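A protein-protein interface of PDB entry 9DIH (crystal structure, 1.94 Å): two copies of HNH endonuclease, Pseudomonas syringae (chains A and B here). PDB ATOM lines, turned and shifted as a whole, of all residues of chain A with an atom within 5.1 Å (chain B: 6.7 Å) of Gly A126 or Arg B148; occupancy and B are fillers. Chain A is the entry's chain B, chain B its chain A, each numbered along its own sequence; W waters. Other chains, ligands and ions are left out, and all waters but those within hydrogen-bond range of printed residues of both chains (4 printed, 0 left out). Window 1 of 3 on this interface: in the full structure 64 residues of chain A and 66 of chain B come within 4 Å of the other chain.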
ATOM      1  N   LEU A 119     -34.683 -11.595  -7.419  1.00  0.00           N
ATOM      2  CA  LEU A 119     -33.332 -12.125  -7.118  1.00  0.00           C
ATOM      3  C   LEU A 119     -32.499 -12.139  -8.370  1.00  0.00           C
ATOM      4  O   LEU A 119     -31.278 -11.885  -8.324  1.00  0.00           O
ATOM      5  CB  LEU A 119     -33.468 -13.522  -6.476  1.00  0.00           C
ATOM      6  CG  LEU A 119     -32.203 -14.270  -6.167  1.00  0.00           C
ATOM      7  CD1 LEU A 119     -31.417 -13.528  -5.057  1.00  0.00           C
ATOM      8  CD2 LEU A 119     -32.540 -15.687  -5.725  1.00  0.00           C
ATOM      9  N   THR A 122     -31.581  -8.254  -9.255  1.00  0.00           N
ATOM     10  CA  THR A 122     -30.584  -7.657  -8.374  1.00  0.00           C
ATOM     11  C   THR A 122     -29.240  -8.380  -8.427  1.00  0.00           C
ATOM     12  O   THR A 122     -28.269  -7.982  -7.754  1.00  0.00           O
ATOM     13  CB  THR A 122     -31.043  -7.649  -6.900  1.00  0.00           C
ATOM     14  OG1 THR A 122     -31.275  -9.026  -6.456  1.00  0.00           O
ATOM     15  CG2 THR A 122     -32.374  -6.863  -6.767  1.00  0.00           C
ATOM     16  N   THR A 123     -29.113  -9.383  -9.258  1.00  0.00           N
ATOM     17  CA  THR A 123     -27.842 -10.084  -9.312  1.00  0.00           C
ATOM     18  C   THR A 123     -26.604  -9.270  -9.604  1.00  0.00           C
ATOM     19  O   THR A 123     -25.532  -9.589  -9.043  1.00  0.00           O
ATOM     20  CB  THR A 123     -27.986 -11.184 -10.356  1.00  0.00           C
ATOM     21  OG1 THR A 123     -28.868 -12.169  -9.840  1.00  0.00           O
ATOM     22  CG2 THR A 123     -26.628 -11.795 -10.607  1.00  0.00           C
ATOM     23  N   PRO A 124     -26.674  -8.143 -10.320  1.00  0.00           N
ATOM     24  CA  PRO A 124     -25.457  -7.290 -10.449  1.00  0.00           C
ATOM     25  C   PRO A 124     -24.884  -6.815  -9.153  1.00  0.00           C
ATOM     26  O   PRO A 124     -23.655  -6.668  -9.092  1.00  0.00           O
ATOM     27  CB  PRO A 124     -25.954  -6.140 -11.290  1.00  0.00           C
ATOM     28  CG  PRO A 124     -26.936  -6.810 -12.197  1.00  0.00           C
ATOM     29  CD  PRO A 124     -27.664  -7.778 -11.300  1.00  0.00           C
ATOM     30  N   ASP A 125     -25.682  -6.635  -8.071  1.00  0.00           N
ATOM     31  CA  ASP A 125     -25.083  -6.138  -6.828  1.00  0.00           C
ATOM     32  C   ASP A 125     -24.316  -7.243  -6.114  1.00  0.00           C
ATOM     33  O   ASP A 125     -23.596  -6.955  -5.167  1.00  0.00           O
ATOM     34  CB  ASP A 125     -26.126  -5.423  -5.937  1.00  0.00           C
ATOM     35  CG  ASP A 125     -26.878  -6.312  -4.939  1.00  0.00           C
ATOM     36  OD1 ASP A 125     -26.449  -7.413  -4.471  1.00  0.00           O
ATOM     37  OD2 ASP A 125     -27.961  -5.808  -4.538  1.00  0.00           O
ATOM     38  N   GLY A 126     -24.447  -8.460  -6.561  1.00  0.00           N
ATOM     39  CA  GLY A 126     -23.623  -9.532  -6.071  1.00  0.00           C
ATOM     40  C   GLY A 126     -22.252  -9.491  -6.644  1.00  0.00           C
ATOM     41  O   GLY A 126     -21.425 -10.345  -6.302  1.00  0.00           O
ATOM     42  N   GLY A 127     -21.973  -8.513  -7.498  1.00  0.00           N
ATOM     43  CA  GLY A 127     -20.605  -8.347  -7.977  1.00  0.00           C
ATOM     44  C   GLY A 127     -19.711  -7.438  -7.180  1.00  0.00           C
ATOM     45  O   GLY A 127     -18.537  -7.238  -7.545  1.00  0.00           O
ATOM     46  N   ARG A 128     -20.195  -6.878  -6.083  1.00  0.00           N
ATOM     47  CA  ARG A 128     -19.416  -5.950  -5.262  1.00  0.00           C
ATOM     48  C   ARG A 128     -18.116  -6.599  -4.881  1.00  0.00           C
ATOM     49  O   ARG A 128     -18.114  -7.734  -4.348  1.00  0.00           O
ATOM     50  CB  ARG A 128     -20.190  -5.574  -3.959  1.00  0.00           C
ATOM     51  CG  ARG A 128     -21.185  -4.480  -4.117  1.00  0.00           C
ATOM     52  CD  ARG A 128     -21.937  -4.200  -2.838  1.00  0.00           C
ATOM     53  NE  ARG A 128     -21.257  -3.164  -2.032  1.00  0.00           N
ATOM     54  CZ  ARG A 128     -20.482  -3.461  -1.007  1.00  0.00           C
ATOM     55  NH1 ARG A 128     -20.328  -4.726  -0.630  1.00  0.00           N
ATOM     56  NH2 ARG A 128     -19.878  -2.477  -0.352  1.00  0.00           N
ATOM     57  N   THR A 204     -27.961  -6.303  -1.384  1.00  0.00           N
ATOM     58  CA  THR A 204     -29.316  -6.617  -1.003  1.00  0.00           C
ATOM     59  C   THR A 204     -29.376  -7.372   0.302  1.00  0.00           C
ATOM     60  O   THR A 204     -30.355  -7.250   1.015  1.00  0.00           O
ATOM     61  CB  THR A 204     -29.962  -7.410  -2.139  1.00  0.00           C
ATOM     62  OG1 THR A 204     -29.964  -6.586  -3.310  1.00  0.00           O
ATOM     63  CG2 THR A 204     -31.417  -7.762  -1.808  1.00  0.00           C
ATOM     64  N   TYR A 205     -28.341  -8.137   0.639  1.00  0.00           N
ATOM     65  CA  TYR A 205     -28.410  -9.068   1.766  1.00  0.00           C
ATOM     66  C   TYR A 205     -27.352  -8.844   2.798  1.00  0.00           C
ATOM     67  O   TYR A 205     -27.316  -9.590   3.776  1.00  0.00           O
ATOM     68  CB  TYR A 205     -28.310 -10.495   1.244  1.00  0.00           C
ATOM     69  CG  TYR A 205     -29.379 -10.803   0.271  1.00  0.00           C
ATOM     70  CD1 TYR A 205     -30.682 -11.008   0.714  1.00  0.00           C
ATOM     71  CD2 TYR A 205     -29.117 -10.886  -1.083  1.00  0.00           C
ATOM     72  CE1 TYR A 205     -31.663 -11.312  -0.128  1.00  0.00           C
ATOM     73  CE2 TYR A 205     -30.124 -11.168  -1.954  1.00  0.00           C
ATOM     74  CZ  TYR A 205     -31.399 -11.365  -1.467  1.00  0.00           C
ATOM     75  OH  TYR A 205     -32.467 -11.633  -2.300  1.00  0.00           O
ATOM     76  N   ASP A 207     -24.076  -9.115   2.252  1.00  0.00           N
ATOM     77  CA  ASP A 207     -22.964 -10.023   2.009  1.00  0.00           C
ATOM     78  C   ASP A 207     -21.653  -9.263   1.984  1.00  0.00           C
ATOM     79  O   ASP A 207     -21.569  -8.070   1.624  1.00  0.00           O
ATOM     80  CB  ASP A 207     -23.144 -10.755   0.643  1.00  0.00           C
ATOM     81  CG  ASP A 207     -24.056 -11.988   0.697  1.00  0.00           C
ATOM     82  OD1 ASP A 207     -24.266 -12.593   1.824  1.00  0.00           O
ATOM     83  OD2 ASP A 207     -24.537 -12.402  -0.418  1.00  0.00           O
ATOM     84  N   LYS A 234     -16.111 -15.966  -1.495  1.00  0.00           N
ATOM     85  CA  LYS A 234     -16.299 -15.569  -2.879  1.00  0.00           C
ATOM     86  C   LYS A 234     -15.040 -14.812  -3.293  1.00  0.00           C
ATOM     87  O   LYS A 234     -14.774 -13.687  -2.838  1.00  0.00           O
ATOM     88  CB  LYS A 234     -17.572 -14.776  -3.061  1.00  0.00           C
ATOM     89  CG  LYS A 234     -17.825 -14.517  -4.591  1.00  0.00           C
ATOM     90  CD  LYS A 234     -19.206 -13.945  -4.843  1.00  0.00           C
ATOM     91  CE  LYS A 234     -19.259 -13.244  -6.178  1.00  0.00           C
ATOM     92  NZ  LYS A 234     -20.616 -13.118  -6.753  1.00  0.00           N
ATOM     93  N   CYS B  35     -25.936  -2.319 -12.068  1.00  0.00           N
ATOM     94  CA  CYS B  35     -25.747  -2.285 -10.581  1.00  0.00           C
ATOM     95  C   CYS B  35     -26.881  -2.938  -9.815  1.00  0.00           C
ATOM     96  O   CYS B  35     -26.714  -3.181  -8.653  1.00  0.00           O
ATOM     97  CB  CYS B  35     -25.569  -0.866 -10.033  1.00  0.00           C
ATOM     98  SG  CYS B  35     -27.016   0.193 -10.021  1.00  0.00           S
ATOM     99  N   ILE B 133     -27.435 -21.189   6.680  1.00  0.00           N
ATOM    100  CA  ILE B 133     -25.975 -21.231   6.487  1.00  0.00           C
ATOM    101  C   ILE B 133     -25.329 -21.475   7.832  1.00  0.00           C
ATOM    102  O   ILE B 133     -25.653 -20.798   8.802  1.00  0.00           O
ATOM    103  CB  ILE B 133     -25.441 -19.928   5.901  1.00  0.00           C
ATOM    104  CG1 ILE B 133     -25.853 -19.785   4.451  1.00  0.00           C
ATOM    105  CG2 ILE B 133     -23.936 -19.933   5.880  1.00  0.00           C
ATOM    106  CD1 ILE B 133     -25.697 -18.427   3.984  1.00  0.00           C
ATOM    107  N   ILE B 145     -19.788 -17.920   3.430  1.00  0.00           N
ATOM    108  CA  ILE B 145     -20.699 -18.350   2.378  1.00  0.00           C
ATOM    109  C   ILE B 145     -21.640 -17.190   2.075  1.00  0.00           C
ATOM    110  O   ILE B 145     -22.398 -16.777   2.967  1.00  0.00           O
ATOM    111  CB  ILE B 145     -21.497 -19.571   2.837  1.00  0.00           C
ATOM    112  CG1 ILE B 145     -20.573 -20.692   3.200  1.00  0.00           C
ATOM    113  CG2 ILE B 145     -22.457 -19.995   1.743  1.00  0.00           C
ATOM    114  CD1 ILE B 145     -21.329 -21.927   3.744  1.00  0.00           C
ATOM    115  N   PRO B 146     -21.687 -16.695   0.854  1.00  0.00           N
ATOM    116  CA  PRO B 146     -22.596 -15.576   0.562  1.00  0.00           C
ATOM    117  C   PRO B 146     -24.052 -16.015   0.652  1.00  0.00           C
ATOM    118  O   PRO B 146     -24.467 -17.065   0.147  1.00  0.00           O
ATOM    119  CB  PRO B 146     -22.240 -15.177  -0.870  1.00  0.00           C
ATOM    120  CG  PRO B 146     -20.956 -15.831  -1.147  1.00  0.00           C
ATOM    121  CD  PRO B 146     -20.927 -17.086  -0.327  1.00  0.00           C
ATOM    122  N   VAL B 147     -24.880 -15.174   1.277  1.00  0.00           N
ATOM    123  CA  VAL B 147     -26.315 -15.465   1.279  1.00  0.00           C
ATOM    124  C   VAL B 147     -26.899 -15.451  -0.124  1.00  0.00           C
ATOM    125  O   VAL B 147     -27.673 -16.334  -0.482  1.00  0.00           O
ATOM    126  CB  VAL B 147     -27.050 -14.437   2.182  1.00  0.00           C
ATOM    127  CG1 VAL B 147     -28.562 -14.565   2.100  1.00  0.00           C
ATOM    128  CG2 VAL B 147     -26.552 -14.583   3.621  1.00  0.00           C
ATOM    129  N   ARG B 148     -26.510 -14.472  -0.956  1.00  0.00           N
ATOM    130  CA  ARG B 148     -27.086 -14.415  -2.292  1.00  0.00           C
ATOM    131  C   ARG B 148     -26.858 -15.705  -3.030  1.00  0.00           C
ATOM    132  O   ARG B 148     -27.722 -16.163  -3.842  1.00  0.00           O
ATOM    133  CB  ARG B 148     -26.534 -13.246  -3.107  1.00  0.00           C
ATOM    134  CG  ARG B 148     -26.966 -13.268  -4.584  1.00  0.00           C
ATOM    135  CD  ARG B 148     -26.508 -12.023  -5.404  1.00  0.00           C
ATOM    136  NE  ARG B 148     -27.169 -10.812  -4.934  1.00  0.00           N
ATOM    137  CZ  ARG B 148     -28.377 -10.417  -5.315  1.00  0.00           C
ATOM    138  NH1 ARG B 148     -29.103 -11.133  -6.131  1.00  0.00           N
ATOM    139  NH2 ARG B 148     -28.884  -9.262  -4.835  1.00  0.00           N
ATOM    140  N   ASP B 149     -25.738 -16.356  -2.802  1.00  0.00           N
ATOM    141  CA  ASP B 149     -25.467 -17.564  -3.603  1.00  0.00           C
ATOM    142  C   ASP B 149     -26.333 -18.727  -3.171  1.00  0.00           C
ATOM    143  O   ASP B 149     -26.711 -19.553  -4.019  1.00  0.00           O
ATOM    144  CB  ASP B 149     -23.982 -17.885  -3.526  1.00  0.00           C
ATOM    145  CG  ASP B 149     -23.140 -16.942  -4.348  1.00  0.00           C
ATOM    146  OD1 ASP B 149     -22.906 -15.792  -3.887  1.00  0.00           O
ATOM    147  OD2 ASP B 149     -22.769 -17.297  -5.507  1.00  0.00           O
ATOM    148  N   LEU B 150     -26.671 -18.837  -1.885  1.00  0.00           N
ATOM    149  CA  LEU B 150     -27.632 -19.908  -1.478  1.00  0.00           C
ATOM    150  C   LEU B 150     -29.018 -19.630  -1.993  1.00  0.00           C
ATOM    151  O   LEU B 150     -29.659 -20.498  -2.607  1.00  0.00           O
ATOM    152  CB  LEU B 150     -27.705 -20.036   0.028  1.00  0.00           C
ATOM    153  CG  LEU B 150     -28.728 -20.993   0.569  1.00  0.00           C
ATOM    154  CD1 LEU B 150     -28.536 -22.413  -0.041  1.00  0.00           C
ATOM    155  CD2 LEU B 150     -28.688 -20.984   2.102  1.00  0.00           C
ATOM    156  N   LEU B 151     -29.483 -18.380  -1.827  1.00  0.00           N
ATOM    157  CA  LEU B 151     -30.812 -18.063  -2.333  1.00  0.00           C
ATOM    158  C   LEU B 151     -30.932 -18.257  -3.823  1.00  0.00           C
ATOM    159  O   LEU B 151     -32.026 -18.604  -4.338  1.00  0.00           O
ATOM    160  CB  LEU B 151     -31.146 -16.610  -1.991  1.00  0.00           C
ATOM    161  CG  LEU B 151     -31.288 -16.274  -0.497  1.00  0.00           C
ATOM    162  CD1 LEU B 151     -31.391 -14.786  -0.369  1.00  0.00           C
ATOM    163  CD2 LEU B 151     -32.471 -16.905   0.059  1.00  0.00           C
ATOM    164  N   THR B 152     -29.832 -18.047  -4.548  1.00  0.00           N
ATOM    165  CA  THR B 152     -29.832 -18.206  -6.020  1.00  0.00           C
ATOM    166  C   THR B 152     -29.834 -19.678  -6.393  1.00  0.00           C
ATOM    167  O   THR B 152     -30.460 -20.096  -7.370  1.00  0.00           O
ATOM    168  CB  THR B 152     -28.559 -17.504  -6.580  1.00  0.00           C
ATOM    169  OG1 THR B 152     -28.599 -16.079  -6.352  1.00  0.00           O
ATOM    170  CG2 THR B 152     -28.419 -17.681  -8.036  1.00  0.00           C
ATOM    171  N   ALA B 153     -29.089 -20.491  -5.636  1.00  0.00           N
ATOM    172  CA  ALA B 153     -29.161 -21.938  -5.856  1.00  0.00           C
ATOM    173  C   ALA B 153     -30.541 -22.484  -5.513  1.00  0.00           C
ATOM    174  O   ALA B 153     -31.084 -23.358  -6.199  1.00  0.00           O
ATOM    175  CB  ALA B 153     -28.061 -22.602  -5.021  1.00  0.00           C
HETATM  176  O   HOH W   1     -21.528 -15.824  -7.343  1.00  0.00           O
HETATM  177  O   HOH W   2     -28.499 -13.396  -7.592  1.00  0.00           O
HETATM  178  O   HOH W   3     -22.947 -13.233  -4.580  1.00  0.00           O
HETATM  179  O   HOH W   4     -25.347  -9.491  -2.863  1.00  0.00           O
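OG1 of Thr A204 lies within hydrogen-bond range of OD2 of Asp A125, at 2.5 Å.
The backbone carbonyl oxygen of Gly A126 is in hydrogen-bond range of the side-chain amino group of Lys A234 (2.9 Å).
The backbone carbonyl oxygen (O) of Leu A119 sits at hydrogen-bond distance from the side-chain hydroxyl (OG1) of Thr A123, at 2.9 Å.
The backbone carbonyl oxygen (O) of Leu A119 lies within hydrogen-bond range of the side-chain hydroxyl (OG1) of Thr A122 (3.4 Å).
The backbone carbonyl oxygen (O) of Arg B148 lies within hydrogen-bond range of the side-chain hydroxyl (OG1) of Thr B152, at 2.7 Å.
Among the printed residues, merely in contact across the chains: Leu A119 with Leu B151 (3.3 Å), Tyr A205 with Leu B151 (3.5 Å), Asp A125 with Cys B35 (3.6 Å), Thr A123 with Arg B148 (3.6 Å), Asp A207 with Pro B146 (3.6 Å), Pro A124 with Cys B35 (3.6 Å), Tyr A205 with Arg B148 (3.7 Å), Leu A119 with Thr B152 (3.7 Å) and Gly A126 with Arg B148 (3.9 Å).
N of Val B147 lies within hydrogen-bond range of OD1 of Asp A207 (2.7 Å).
NH2 of Arg B148 is in salt-bridge range of OD1 of Asp A125 (3.1 Å).
NH2 of Arg B148 is in hydrogen-bond range of OG1 of Thr A204.
The side-chain carboxylate (OD2) of Asp A207 sits at hydrogen-bond distance from the backbone NH (N) of Arg B148, 2.9 Å away.
NH2 of Arg B148 is in hydrogen-bond range of OG1 of Thr A122 (2.9 Å).
O of Leu A119 is in hydrogen-bond range of NH1 of Arg B148.
Along chain A the printed residues that touch a printed residue of chain B span positions 119 to 207.
Of the 11 printed residues of chain B, 6 touch a printed residue of chain A.
Printed residues of chain B that touch a printed residue of chain A: Cys B35, Pro B146, Val B147, Arg B148, Leu B151 and Thr B152.
Hydrophobic or aromatic side chains of chain B that line the printed part of chain A: Pro B146, Val B147 and Leu B151.
Among the printed residues, 15 pairs touch across the chains.
Among the printed residues, Asp or Glu carboxylates within 4 Å of a Lys or Arg side-chain nitrogen of the other chain: Asp A125 with Arg B148 (3.1 Å).
Gly A126 touches just one residue of chain B: Arg B148 (3.9 Å).
Of the printed residues of chain A, Arg B148 touches Leu A119 (3.2 Å), Thr A122 (2.9 Å), Thr A123 (3.6 Å), Asp A125 (3.1 Å), Gly A126 (3.9 Å), Thr A204 (3.3 Å), Tyr A205 (3.7 Å) and Asp A207 (2.9 Å).
Of the printed residues of chain A, Thr B152 touches Leu A119.
Printed residues of chain A within 4 Å of Leu B151: Leu A119 (3.3 Å) and Tyr A205 (3.5 Å).
Asp B149 touches none of the printed residues of chain A.
The nearest printed residue of chain A that does not touch Pro B146 is Lys A234 (4.03 Å).
Water W2 lies within hydrogen-bond range of the side-chain hydroxyl of Thr A123 (2.6 Å), the guanidinium group of Arg B148 (2.8 Å), the side-chain hydroxyl of Thr B152 (3.0 Å) and the backbone carbonyl oxygen of Leu A119 (3.2 Å).
Water W3 bridges OD1 of Asp B149 (2.7 Å) and NZ of Lys A234 (3.2 Å).
Water W1 lies within hydrogen-bond range of the side-chain carboxylate (OD2) of Asp B149 (2.7 Å) and the side-chain amino group (NZ) of Lys A234 (2.9 Å).
Water W4 lies within hydrogen-bond range of OD1 of Asp A125 (2.8 Å) and NE of Arg B148 (3.1 Å).
No position is printed for both chains.
Of the 15 pairs that touch across the chains among the printed residues, none has its exchanged pair printed and touching as well.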
